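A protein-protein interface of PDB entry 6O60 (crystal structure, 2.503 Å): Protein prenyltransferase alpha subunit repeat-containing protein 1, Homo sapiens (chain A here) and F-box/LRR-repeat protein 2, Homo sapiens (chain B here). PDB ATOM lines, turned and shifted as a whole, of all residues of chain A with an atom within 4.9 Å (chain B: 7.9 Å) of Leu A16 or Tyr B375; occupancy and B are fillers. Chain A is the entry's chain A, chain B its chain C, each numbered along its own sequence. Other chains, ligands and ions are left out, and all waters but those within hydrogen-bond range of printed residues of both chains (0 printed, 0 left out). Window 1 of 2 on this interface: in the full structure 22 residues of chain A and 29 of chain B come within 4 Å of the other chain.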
ATOM      1  N   GLU A  12     -10.205 -21.015  31.046  1.00  0.00           N
ATOM      2  CA  GLU A  12      -9.878 -20.097  29.970  1.00  0.00           C
ATOM      3  C   GLU A  12      -9.707 -18.672  30.479  1.00  0.00           C
ATOM      4  O   GLU A  12      -9.080 -17.854  29.801  1.00  0.00           O
ATOM      5  CB  GLU A  12     -10.948 -20.143  28.875  1.00  0.00           C
ATOM      6  CG  GLU A  12     -10.769 -21.301  27.877  1.00  0.00           C
ATOM      7  CD  GLU A  12     -11.222 -21.000  26.427  1.00  0.00           C
ATOM      8  OE1 GLU A  12     -10.864 -21.798  25.531  1.00  0.00           O
ATOM      9  OE2 GLU A  12     -11.942 -20.001  26.178  1.00  0.00           O
ATOM     10  N   VAL A  13     -10.254 -18.342  31.647  1.00  0.00           N
ATOM     11  CA  VAL A  13     -10.125 -16.970  32.126  1.00  0.00           C
ATOM     12  C   VAL A  13      -8.741 -16.745  32.704  1.00  0.00           C
ATOM     13  O   VAL A  13      -8.134 -15.683  32.497  1.00  0.00           O
ATOM     14  CB  VAL A  13     -11.226 -16.648  33.149  1.00  0.00           C
ATOM     15  CG1 VAL A  13     -11.314 -17.741  34.171  1.00  0.00           C
ATOM     16  CG2 VAL A  13     -10.934 -15.330  33.835  1.00  0.00           C
ATOM     17  N   ALA A  14      -8.215 -17.754  33.409  1.00  0.00           N
ATOM     18  CA  ALA A  14      -6.862 -17.686  33.943  1.00  0.00           C
ATOM     19  C   ALA A  14      -5.867 -17.367  32.847  1.00  0.00           C
ATOM     20  O   ALA A  14      -4.967 -16.541  33.035  1.00  0.00           O
ATOM     21  CB  ALA A  14      -6.499 -19.005  34.620  1.00  0.00           C
ATOM     22  N   VAL A  15      -6.012 -18.017  31.690  1.00  0.00           N
ATOM     23  CA  VAL A  15      -5.130 -17.724  30.563  1.00  0.00           C
ATOM     24  C   VAL A  15      -5.306 -16.278  30.137  1.00  0.00           C
ATOM     25  O   VAL A  15      -4.337 -15.537  29.950  1.00  0.00           O
ATOM     26  CB  VAL A  15      -5.406 -18.692  29.401  1.00  0.00           C
ATOM     27  CG1 VAL A  15      -4.536 -18.335  28.208  1.00  0.00           C
ATOM     28  CG2 VAL A  15      -5.173 -20.135  29.844  1.00  0.00           C
ATOM     29  N   LEU A  16      -6.557 -15.845  30.027  1.00  0.00           N
ATOM     30  CA  LEU A  16      -6.831 -14.480  29.618  1.00  0.00           C
ATOM     31  C   LEU A  16      -6.250 -13.469  30.606  1.00  0.00           C
ATOM     32  O   LEU A  16      -5.663 -12.459  30.199  1.00  0.00           O
ATOM     33  CB  LEU A  16      -8.334 -14.296  29.463  1.00  0.00           C
ATOM     34  CG  LEU A  16      -8.719 -12.914  28.967  1.00  0.00           C
ATOM     35  CD1 LEU A  16      -9.602 -13.068  27.753  1.00  0.00           C
ATOM     36  CD2 LEU A  16      -9.451 -12.173  30.081  1.00  0.00           C
ATOM     37  N   VAL A  17      -6.396 -13.716  31.907  1.00  0.00           N
ATOM     38  CA  VAL A  17      -5.882 -12.734  32.855  1.00  0.00           C
ATOM     39  C   VAL A  17      -4.361 -12.654  32.770  1.00  0.00           C
ATOM     40  O   VAL A  17      -3.789 -11.559  32.786  1.00  0.00           O
ATOM     41  CB  VAL A  17      -6.369 -13.035  34.285  1.00  0.00           C
ATOM     42  CG1 VAL A  17      -5.707 -12.074  35.224  1.00  0.00           C
ATOM     43  CG2 VAL A  17      -7.874 -12.852  34.393  1.00  0.00           C
ATOM     44  N   GLN A  18      -3.688 -13.804  32.654  1.00  0.00           N
ATOM     45  CA  GLN A  18      -2.243 -13.811  32.448  1.00  0.00           C
ATOM     46  C   GLN A  18      -1.869 -13.024  31.206  1.00  0.00           C
ATOM     47  O   GLN A  18      -0.895 -12.262  31.203  1.00  0.00           O
ATOM     48  CB  GLN A  18      -1.739 -15.247  32.319  1.00  0.00           C
ATOM     49  CG  GLN A  18      -1.738 -15.998  33.621  1.00  0.00           C
ATOM     50  CD  GLN A  18      -1.315 -17.429  33.451  1.00  0.00           C
ATOM     51  OE1 GLN A  18      -1.989 -18.342  33.936  1.00  0.00           O
ATOM     52  NE2 GLN A  18      -0.184 -17.644  32.766  1.00  0.00           N
ATOM     53  N   ARG A  19      -2.636 -13.212  30.138  1.00  0.00           N
ATOM     54  CA  ARG A  19      -2.402 -12.477  28.912  1.00  0.00           C
ATOM     55  C   ARG A  19      -2.513 -10.977  29.145  1.00  0.00           C
ATOM     56  O   ARG A  19      -1.687 -10.199  28.655  1.00  0.00           O
ATOM     57  CB  ARG A  19      -3.400 -12.943  27.850  1.00  0.00           C
ATOM     58  CG  ARG A  19      -3.298 -12.164  26.578  1.00  0.00           C
ATOM     59  CD  ARG A  19      -1.867 -12.062  26.170  1.00  0.00           C
ATOM     60  NE  ARG A  19      -1.729 -11.952  24.731  1.00  0.00           N
ATOM     61  CZ  ARG A  19      -0.721 -11.316  24.149  1.00  0.00           C
ATOM     62  NH1 ARG A  19      -0.657 -11.235  22.831  1.00  0.00           N
ATOM     63  NH2 ARG A  19       0.232 -10.768  24.897  1.00  0.00           N
ATOM     64  N   VAL A  20      -3.527 -10.551  29.898  1.00  0.00           N
ATOM     65  CA  VAL A  20      -3.739  -9.125  30.102  1.00  0.00           C
ATOM     66  C   VAL A  20      -2.661  -8.556  31.009  1.00  0.00           C
ATOM     67  O   VAL A  20      -2.175  -7.443  30.791  1.00  0.00           O
ATOM     68  CB  VAL A  20      -5.165  -8.879  30.627  1.00  0.00           C
ATOM     69  CG1 VAL A  20      -5.373  -7.408  30.982  1.00  0.00           C
ATOM     70  CG2 VAL A  20      -6.162  -9.340  29.568  1.00  0.00           C
ATOM     71  N   ASN A  48     -10.830  -9.085  18.535  1.00  0.00           N
ATOM     72  CA  ASN A  48      -9.649  -9.763  19.069  1.00  0.00           C
ATOM     73  C   ASN A  48      -8.475  -8.790  19.214  1.00  0.00           C
ATOM     74  O   ASN A  48      -7.397  -8.985  18.653  1.00  0.00           O
ATOM     75  CB  ASN A  48      -9.278 -10.946  18.185  1.00  0.00           C
ATOM     76  CG  ASN A  48      -8.220 -11.838  18.817  1.00  0.00           C
ATOM     77  OD1 ASN A  48      -8.041 -11.857  20.047  1.00  0.00           O
ATOM     78  ND2 ASN A  48      -7.520 -12.592  17.979  1.00  0.00           N
ATOM     79  N   TRP A  64     -14.387  -4.372  30.335  1.00  0.00           N
ATOM     80  CA  TRP A  64     -14.953  -5.719  30.288  1.00  0.00           C
ATOM     81  C   TRP A  64     -14.061  -6.759  30.943  1.00  0.00           C
ATOM     82  O   TRP A  64     -14.573  -7.791  31.386  1.00  0.00           O
ATOM     83  CB  TRP A  64     -15.249  -6.135  28.849  1.00  0.00           C
ATOM     84  CG  TRP A  64     -14.077  -6.181  27.944  1.00  0.00           C
ATOM     85  CD1 TRP A  64     -13.601  -5.165  27.147  1.00  0.00           C
ATOM     86  CD2 TRP A  64     -13.234  -7.310  27.697  1.00  0.00           C
ATOM     87  NE1 TRP A  64     -12.511  -5.598  26.433  1.00  0.00           N
ATOM     88  CE2 TRP A  64     -12.262  -6.907  26.754  1.00  0.00           C
ATOM     89  CE3 TRP A  64     -13.202  -8.621  28.183  1.00  0.00           C
ATOM     90  CZ2 TRP A  64     -11.278  -7.767  26.290  1.00  0.00           C
ATOM     91  CZ3 TRP A  64     -12.219  -9.474  27.718  1.00  0.00           C
ATOM     92  CH2 TRP A  64     -11.272  -9.043  26.782  1.00  0.00           C
ATOM     93  N   PHE A  68     -12.600  -9.881  35.615  1.00  0.00           N
ATOM     94  CA  PHE A  68     -11.811 -11.102  35.675  1.00  0.00           C
ATOM     95  C   PHE A  68     -10.436 -10.843  36.262  1.00  0.00           C
ATOM     96  O   PHE A  68      -9.909 -11.665  37.018  1.00  0.00           O
ATOM     97  CB  PHE A  68     -11.638 -11.704  34.276  1.00  0.00           C
ATOM     98  CG  PHE A  68     -12.925 -11.965  33.553  1.00  0.00           C
ATOM     99  CD1 PHE A  68     -13.799 -12.954  33.996  1.00  0.00           C
ATOM    100  CD2 PHE A  68     -13.258 -11.227  32.420  1.00  0.00           C
ATOM    101  CE1 PHE A  68     -14.979 -13.201  33.329  1.00  0.00           C
ATOM    102  CE2 PHE A  68     -14.442 -11.468  31.743  1.00  0.00           C
ATOM    103  CZ  PHE A  68     -15.308 -12.456  32.198  1.00  0.00           C
ATOM    104  N   SER B 321       4.867 -15.348  18.921  1.00  0.00           N
ATOM    105  CA  SER B 321       4.290 -14.078  19.351  1.00  0.00           C
ATOM    106  C   SER B 321       5.092 -12.908  18.803  1.00  0.00           C
ATOM    107  O   SER B 321       6.326 -12.919  18.844  1.00  0.00           O
ATOM    108  CB  SER B 321       4.240 -13.991  20.875  1.00  0.00           C
ATOM    109  OG  SER B 321       3.277 -14.878  21.402  1.00  0.00           O
ATOM    110  N   HIS B 322       4.370 -11.911  18.260  1.00  0.00           N
ATOM    111  CA  HIS B 322       4.935 -10.679  17.710  1.00  0.00           C
ATOM    112  C   HIS B 322       5.815 -10.907  16.486  1.00  0.00           C
ATOM    113  O   HIS B 322       6.405  -9.961  15.958  1.00  0.00           O
ATOM    114  CB  HIS B 322       5.727  -9.935  18.784  1.00  0.00           C
ATOM    115  CG  HIS B 322       4.884  -9.479  19.929  1.00  0.00           C
ATOM    116  ND1 HIS B 322       4.164  -8.304  19.900  1.00  0.00           N
ATOM    117  CD2 HIS B 322       4.625 -10.053  21.129  1.00  0.00           C
ATOM    118  CE1 HIS B 322       3.512  -8.166  21.041  1.00  0.00           C
ATOM    119  NE2 HIS B 322       3.775  -9.213  21.805  1.00  0.00           N
ATOM    120  N   GLU B 348       1.621 -20.596  19.621  1.00  0.00           N
ATOM    121  CA  GLU B 348       1.301 -19.249  20.085  1.00  0.00           C
ATOM    122  C   GLU B 348       1.572 -18.289  18.941  1.00  0.00           C
ATOM    123  O   GLU B 348       2.726 -18.092  18.557  1.00  0.00           O
ATOM    124  CB  GLU B 348       2.113 -18.890  21.328  1.00  0.00           C
ATOM    125  CG  GLU B 348       2.363 -20.085  22.245  1.00  0.00           C
ATOM    126  CD  GLU B 348       2.534 -19.708  23.709  1.00  0.00           C
ATOM    127  OE1 GLU B 348       1.871 -18.754  24.167  1.00  0.00           O
ATOM    128  OE2 GLU B 348       3.329 -20.369  24.407  1.00  0.00           O
ATOM    129  N   LEU B 349       0.511 -17.700  18.391  1.00  0.00           N
ATOM    130  CA  LEU B 349       0.638 -16.804  17.246  1.00  0.00           C
ATOM    131  C   LEU B 349       0.158 -15.396  17.549  1.00  0.00           C
ATOM    132  O   LEU B 349      -0.204 -14.668  16.629  1.00  0.00           O
ATOM    133  CB  LEU B 349      -0.123 -17.346  16.034  1.00  0.00           C
ATOM    134  CG  LEU B 349       0.111 -18.789  15.584  1.00  0.00           C
ATOM    135  CD1 LEU B 349      -0.920 -19.136  14.534  1.00  0.00           C
ATOM    136  CD2 LEU B 349       1.523 -19.029  15.065  1.00  0.00           C
ATOM    137  N   ASP B 350       0.157 -14.979  18.805  1.00  0.00           N
ATOM    138  CA  ASP B 350      -0.444 -13.692  19.114  1.00  0.00           C
ATOM    139  C   ASP B 350       0.424 -12.545  18.617  1.00  0.00           C
ATOM    140  O   ASP B 350       1.648 -12.646  18.538  1.00  0.00           O
ATOM    141  CB  ASP B 350      -0.712 -13.556  20.612  1.00  0.00           C
ATOM    142  CG  ASP B 350       0.409 -14.081  21.453  1.00  0.00           C
ATOM    143  OD1 ASP B 350       0.576 -15.320  21.496  1.00  0.00           O
ATOM    144  OD2 ASP B 350       1.124 -13.252  22.060  1.00  0.00           O
ATOM    145  N   ASN B 351      -0.251 -11.456  18.253  1.00  0.00           N
ATOM    146  CA  ASN B 351       0.304 -10.269  17.602  1.00  0.00           C
ATOM    147  C   ASN B 351       0.986 -10.594  16.284  1.00  0.00           C
ATOM    148  O   ASN B 351       1.751  -9.772  15.764  1.00  0.00           O
ATOM    149  CB  ASN B 351       1.244  -9.490  18.524  1.00  0.00           C
ATOM    150  CG  ASN B 351       0.524  -8.932  19.747  1.00  0.00           C
ATOM    151  OD1 ASN B 351       0.445  -9.589  20.787  1.00  0.00           O
ATOM    152  ND2 ASN B 351      -0.007  -7.720  19.625  1.00  0.00           N
ATOM    153  N   CYS B 352       0.711 -11.784  15.743  1.00  0.00           N
ATOM    154  CA  CYS B 352       0.929 -12.081  14.330  1.00  0.00           C
ATOM    155  C   CYS B 352      -0.265 -11.519  13.569  1.00  0.00           C
ATOM    156  O   CYS B 352      -1.280 -12.191  13.352  1.00  0.00           O
ATOM    157  CB  CYS B 352       1.110 -13.574  14.115  1.00  0.00           C
ATOM    158  SG  CYS B 352       2.593 -14.152  14.952  1.00  0.00           S
ATOM    159  N   LEU B 353      -0.138 -10.256  13.155  1.00  0.00           N
ATOM    160  CA  LEU B 353      -1.283  -9.526  12.627  1.00  0.00           C
ATOM    161  C   LEU B 353      -1.854 -10.119  11.339  1.00  0.00           C
ATOM    162  O   LEU B 353      -3.031  -9.892  11.043  1.00  0.00           O
ATOM    163  CB  LEU B 353      -0.893  -8.063  12.419  1.00  0.00           C
ATOM    164  CG  LEU B 353      -0.915  -7.275  13.739  1.00  0.00           C
ATOM    165  CD1 LEU B 353       0.411  -7.372  14.501  1.00  0.00           C
ATOM    166  CD2 LEU B 353      -1.306  -5.828  13.492  1.00  0.00           C
ATOM    167  N   ARG B 371      -3.476 -26.444  22.827  1.00  0.00           N
ATOM    168  CA  ARG B 371      -3.483 -25.048  23.231  1.00  0.00           C
ATOM    169  C   ARG B 371      -3.084 -24.202  22.035  1.00  0.00           C
ATOM    170  O   ARG B 371      -2.024 -24.416  21.438  1.00  0.00           O
ATOM    171  CB  ARG B 371      -2.531 -24.822  24.408  1.00  0.00           C
ATOM    172  CG  ARG B 371      -2.585 -23.439  25.003  1.00  0.00           C
ATOM    173  CD  ARG B 371      -1.684 -23.315  26.221  1.00  0.00           C
ATOM    174  NE  ARG B 371      -0.901 -22.081  26.175  1.00  0.00           N
ATOM    175  CZ  ARG B 371       0.400 -22.003  26.444  1.00  0.00           C
ATOM    176  NH1 ARG B 371       1.084 -23.093  26.806  1.00  0.00           N
ATOM    177  NH2 ARG B 371       1.016 -20.826  26.359  1.00  0.00           N
ATOM    178  N   LEU B 372      -3.936 -23.250  21.688  1.00  0.00           N
ATOM    179  CA  LEU B 372      -3.670 -22.346  20.584  1.00  0.00           C
ATOM    180  C   LEU B 372      -3.969 -20.940  21.073  1.00  0.00           C
ATOM    181  O   LEU B 372      -5.040 -20.687  21.629  1.00  0.00           O
ATOM    182  CB  LEU B 372      -4.539 -22.696  19.369  1.00  0.00           C
ATOM    183  CG  LEU B 372      -4.109 -22.356  17.941  1.00  0.00           C
ATOM    184  CD1 LEU B 372      -5.238 -22.717  16.990  1.00  0.00           C
ATOM    185  CD2 LEU B 372      -3.679 -20.916  17.766  1.00  0.00           C
ATOM    186  N   GLU B 373      -3.033 -20.027  20.871  1.00  0.00           N
ATOM    187  CA  GLU B 373      -3.183 -18.664  21.347  1.00  0.00           C
ATOM    188  C   GLU B 373      -3.213 -17.716  20.163  1.00  0.00           C
ATOM    189  O   GLU B 373      -2.344 -17.779  19.288  1.00  0.00           O
ATOM    190  CB  GLU B 373      -2.059 -18.311  22.323  1.00  0.00           C
ATOM    191  CG  GLU B 373      -2.081 -19.215  23.534  1.00  0.00           C
ATOM    192  CD  GLU B 373      -1.823 -18.461  24.791  1.00  0.00           C
ATOM    193  OE1 GLU B 373      -1.313 -17.321  24.684  1.00  0.00           O
ATOM    194  OE2 GLU B 373      -2.139 -18.992  25.880  1.00  0.00           O
ATOM    195  N   LEU B 374      -4.220 -16.842  20.140  1.00  0.00           N
ATOM    196  CA  LEU B 374      -4.456 -15.971  18.999  1.00  0.00           C
ATOM    197  C   LEU B 374      -4.688 -14.520  19.394  1.00  0.00           C
ATOM    198  O   LEU B 374      -5.099 -13.732  18.545  1.00  0.00           O
ATOM    199  CB  LEU B 374      -5.645 -16.479  18.180  1.00  0.00           C
ATOM    200  CG  LEU B 374      -5.501 -17.883  17.588  1.00  0.00           C
ATOM    201  CD1 LEU B 374      -6.874 -18.466  17.332  1.00  0.00           C
ATOM    202  CD2 LEU B 374      -4.658 -17.858  16.301  1.00  0.00           C
ATOM    203  N   TYR B 375      -4.425 -14.148  20.646  1.00  0.00           N
ATOM    204  CA  TYR B 375      -4.536 -12.764  21.102  1.00  0.00           C
ATOM    205  C   TYR B 375      -4.012 -11.767  20.070  1.00  0.00           C
ATOM    206  O   TYR B 375      -2.981 -11.987  19.436  1.00  0.00           O
ATOM    207  CB  TYR B 375      -3.770 -12.610  22.423  1.00  0.00           C
ATOM    208  CG  TYR B 375      -4.374 -13.433  23.536  1.00  0.00           C
ATOM    209  CD1 TYR B 375      -5.634 -13.099  24.067  1.00  0.00           C
ATOM    210  CD2 TYR B 375      -3.718 -14.562  24.035  1.00  0.00           C
ATOM    211  CE1 TYR B 375      -6.214 -13.855  25.068  1.00  0.00           C
ATOM    212  CE2 TYR B 375      -4.291 -15.334  25.057  1.00  0.00           C
ATOM    213  CZ  TYR B 375      -5.541 -14.972  25.568  1.00  0.00           C
ATOM    214  OH  TYR B 375      -6.123 -15.717  26.572  1.00  0.00           O
ATOM    215  N   ASP B 376      -4.752 -10.679  19.883  1.00  0.00           N
ATOM    216  CA  ASP B 376      -4.355  -9.561  19.026  1.00  0.00           C
ATOM    217  C   ASP B 376      -4.215  -9.942  17.545  1.00  0.00           C
ATOM    218  O   ASP B 376      -3.730  -9.131  16.746  1.00  0.00           O
ATOM    219  CB  ASP B 376      -3.058  -8.912  19.539  1.00  0.00           C
ATOM    220  CG  ASP B 376      -3.321  -7.854  20.596  1.00  0.00           C
ATOM    221  OD1 ASP B 376      -4.194  -6.997  20.366  1.00  0.00           O
ATOM    222  OD2 ASP B 376      -2.666  -7.872  21.661  1.00  0.00           O
ATOM    223  N   CYS B 377      -4.618 -11.158  17.160  1.00  0.00           N
ATOM    224  CA  CYS B 377      -4.749 -11.544  15.760  1.00  0.00           C
ATOM    225  C   CYS B 377      -6.120 -11.093  15.262  1.00  0.00           C
ATOM    226  O   CYS B 377      -7.093 -11.850  15.235  1.00  0.00           O
ATOM    227  CB  CYS B 377      -4.572 -13.043  15.602  1.00  0.00           C
ATOM    228  SG  CYS B 377      -2.904 -13.635  15.743  1.00  0.00           S
ATOM    229  N   GLN B 378      -6.181  -9.828  14.843  1.00  0.00           N
ATOM    230  CA  GLN B 378      -7.465  -9.187  14.586  1.00  0.00           C
ATOM    231  C   GLN B 378      -8.181  -9.700  13.341  1.00  0.00           C
ATOM    232  O   GLN B 378      -9.390  -9.487  13.225  1.00  0.00           O
ATOM    233  CB  GLN B 378      -7.268  -7.689  14.473  1.00  0.00           C
ATOM    234  CG  GLN B 378      -7.263  -7.027  15.811  1.00  0.00           C
ATOM    235  CD  GLN B 378      -6.520  -5.719  15.805  1.00  0.00           C
ATOM    236  OE1 GLN B 378      -7.103  -4.671  15.524  1.00  0.00           O
ATOM    237  NE2 GLN B 378      -5.236  -5.758  16.171  1.00  0.00           N
ATOM    238  N   VAL B 380      -8.826 -12.694  12.765  1.00  0.00           N
ATOM    239  CA  VAL B 380      -9.451 -13.957  13.138  1.00  0.00           C
ATOM    240  C   VAL B 380     -10.836 -13.680  13.728  1.00  0.00           C
ATOM    241  O   VAL B 380     -10.979 -12.874  14.659  1.00  0.00           O
ATOM    242  CB  VAL B 380      -8.555 -14.719  14.131  1.00  0.00           C
ATOM    243  CG1 VAL B 380      -9.214 -15.995  14.576  1.00  0.00           C
ATOM    244  CG2 VAL B 380      -7.178 -14.994  13.510  1.00  0.00           C
ATOM    245  N   VAL B 397      -8.470 -22.870  22.392  1.00  0.00           N
ATOM    246  CA  VAL B 397      -7.924 -21.754  21.636  1.00  0.00           C
ATOM    247  C   VAL B 397      -8.238 -20.495  22.420  1.00  0.00           C
ATOM    248  O   VAL B 397      -9.282 -20.395  23.072  1.00  0.00           O
ATOM    249  CB  VAL B 397      -8.458 -21.718  20.181  1.00  0.00           C
ATOM    250  CG1 VAL B 397      -9.606 -22.690  19.999  1.00  0.00           C
ATOM    251  CG2 VAL B 397      -8.846 -20.321  19.761  1.00  0.00           C
ATOM    252  N   HIS B 398      -7.311 -19.541  22.407  1.00  0.00           N
ATOM    253  CA  HIS B 398      -7.382 -18.402  23.317  1.00  0.00           C
ATOM    254  C   HIS B 398      -7.263 -17.089  22.558  1.00  0.00           C
ATOM    255  O   HIS B 398      -6.204 -16.783  22.002  1.00  0.00           O
ATOM    256  CB  HIS B 398      -6.306 -18.519  24.389  1.00  0.00           C
ATOM    257  CG  HIS B 398      -6.526 -19.668  25.316  1.00  0.00           C
ATOM    258  ND1 HIS B 398      -5.556 -20.611  25.581  1.00  0.00           N
ATOM    259  CD2 HIS B 398      -7.620 -20.042  26.026  1.00  0.00           C
ATOM    260  CE1 HIS B 398      -6.036 -21.506  26.427  1.00  0.00           C
ATOM    261  NE2 HIS B 398      -7.284 -21.184  26.715  1.00  0.00           N
ATOM    262  N   ALA B 399      -8.346 -16.313  22.549  1.00  0.00           N
ATOM    263  CA  ALA B 399      -8.344 -14.964  22.003  1.00  0.00           C
ATOM    264  C   ALA B 399      -9.027 -14.041  23.011  1.00  0.00           C
ATOM    265  O   ALA B 399      -9.433 -14.466  24.094  1.00  0.00           O
ATOM    266  CB  ALA B 399      -9.006 -14.930  20.622  1.00  0.00           C
ATOM    267  N   TYR B 400      -9.118 -12.760  22.677  1.00  0.00           N
ATOM    268  CA  TYR B 400      -9.765 -11.813  23.575  1.00  0.00           C
ATOM    269  C   TYR B 400     -11.291 -11.831  23.499  1.00  0.00           C
ATOM    270  O   TYR B 400     -11.925 -11.072  24.242  1.00  0.00           O
ATOM    271  CB  TYR B 400      -9.286 -10.390  23.282  1.00  0.00           C
ATOM    272  CG  TYR B 400      -7.845 -10.128  23.612  1.00  0.00           C
ATOM    273  CD1 TYR B 400      -7.413 -10.061  24.939  1.00  0.00           C
ATOM    274  CD2 TYR B 400      -6.922  -9.910  22.605  1.00  0.00           C
ATOM    275  CE1 TYR B 400      -6.095  -9.811  25.253  1.00  0.00           C
ATOM    276  CE2 TYR B 400      -5.589  -9.664  22.903  1.00  0.00           C
ATOM    277  CZ  TYR B 400      -5.185  -9.618  24.225  1.00  0.00           C
ATOM    278  OH  TYR B 400      -3.884  -9.355  24.509  1.00  0.00           O
ATOM    279  N   PHE B 401     -11.897 -12.659  22.643  1.00  0.00           N
ATOM    280  CA  PHE B 401     -13.358 -12.627  22.435  1.00  0.00           C
ATOM    281  C   PHE B 401     -14.173 -13.016  23.668  1.00  0.00           C
ATOM    282  O   PHE B 401     -14.041 -14.122  24.196  1.00  0.00           O
ATOM    283  CB  PHE B 401     -13.746 -13.537  21.273  1.00  0.00           C
ATOM    284  CG  PHE B 401     -13.424 -12.959  19.920  1.00  0.00           C
ATOM    285  CD1 PHE B 401     -13.858 -11.700  19.575  1.00  0.00           C
ATOM    286  CD2 PHE B 401     -12.677 -13.683  19.002  1.00  0.00           C
ATOM    287  CE1 PHE B 401     -13.572 -11.170  18.322  1.00  0.00           C
ATOM    288  CE2 PHE B 401     -12.386 -13.168  17.761  1.00  0.00           C
ATOM    289  CZ  PHE B 401     -12.830 -11.910  17.415  1.00  0.00           C
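The guanidinium group (NE) of Arg A19 sits at hydrogen-bond distance from the side-chain hydroxyl (OH) of Tyr B400 (3.4 Å). The side-chain amide nitrogen (ND2) of Asn A48 sits at hydrogen-bond distance from the backbone carbonyl oxygen (O) of Leu B374, 2.7 Å away. OH of Tyr B375 lies close to N of Leu A16. The side-chain amide oxygen (OD1) of Asn A48 sits at hydrogen-bond distance from the backbone NH (N) of Tyr B400. O of Cys B377 sits at hydrogen-bond distance from ND2 of Asn A48 (2.9 Å). The side-chain carboxylate (OE1) of Glu A12 sits close to the backbone carbonyl oxygen (O) of Val B397 (3.2 Å). The backbone carbonyl oxygen (O) of Asn A48 sits close to the backbone NH (N) of Asp B376, at 3.4 Å. The guanidinium group of Arg A19 lies within hydrogen-bond range of the side-chain amide oxygen of Asn B351. NH1 of Arg A19 lies within salt-bridge range of OD2 of Asp B350 (2.8 Å).
Leu A16 touches just these residues of chain B: Tyr B375 (3.4 Å) and Ala B399 (3.9 Å). Of the printed residues of chain A, Tyr B375 touches Val A15, Leu A16, Arg A19 and Asn A48. Printed residues of chain A within 4 Å of Val B397: Glu A12 (3.2 Å). Of the printed residues of chain A, Asn B351 touches Arg A19 (2.8 Å). Cys B352 touches none of the printed residues of chain A. Val A17 touches none of the printed residues of chain B. The nearest residue of chain B that does not touch Leu A16 is Tyr B400 (4.4 Å).
N of His B322 sits at hydrogen-bond distance from O of Asp B350. The side-chain sulfur of Cys B377 is in hydrogen-bond range of the backbone carbonyl oxygen of Cys B352 (3.2 Å). OE2 of Glu B373 is in salt-bridge range of NE of Arg B371 (3.3 Å). The backbone carbonyl oxygen (O) of Leu B374 sits close to the side-chain sulfur (SG) of Cys B377 (3.6 Å). The backbone carbonyl oxygen (O) of Glu B373 sits at hydrogen-bond distance from the backbone NH (N) of Leu B349 (3.0 Å). The side-chain amide nitrogen (ND2) of Asn B351 sits close to the side-chain carboxylate (OD2) of Asp B376, at 3.4 Å.
His B398 touches Glu A12. Val A15 touches Glu B373. CG1 of Val A15 touches OH of Tyr B375, at 3.5 Å. His B398 touches Val A15. Tyr B375 touches Arg A19 (CB to NE, 3.2 Å). Asn A48 touches Tyr B375. Asn A48 touches Gln B378 (O to CG, 3.5 Å). Ala B399 touches Asn A48 (CB to OD1, 3.3 Å). CE1 of Phe B401 touches N of Asn A48, at 3.5 Å. CH2 of Trp A64 touches O of Tyr B400, at 3.3 Å.
Of the 12 printed residues of chain A, 6 touch a printed residue of chain B. Hydrophobic or aromatic side chains of chain A within 4 Å of the printed part of chain B: Val A15, Leu A16 and Trp A64. Along chain A the printed residues that touch a printed residue of chain B span positions 12 to 64. Among the printed residues, Asp or Glu carboxylates within 4 Å of a Lys or Arg side-chain nitrogen of the other chain: Arg A19 with Asp B350 (2.8 Å).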
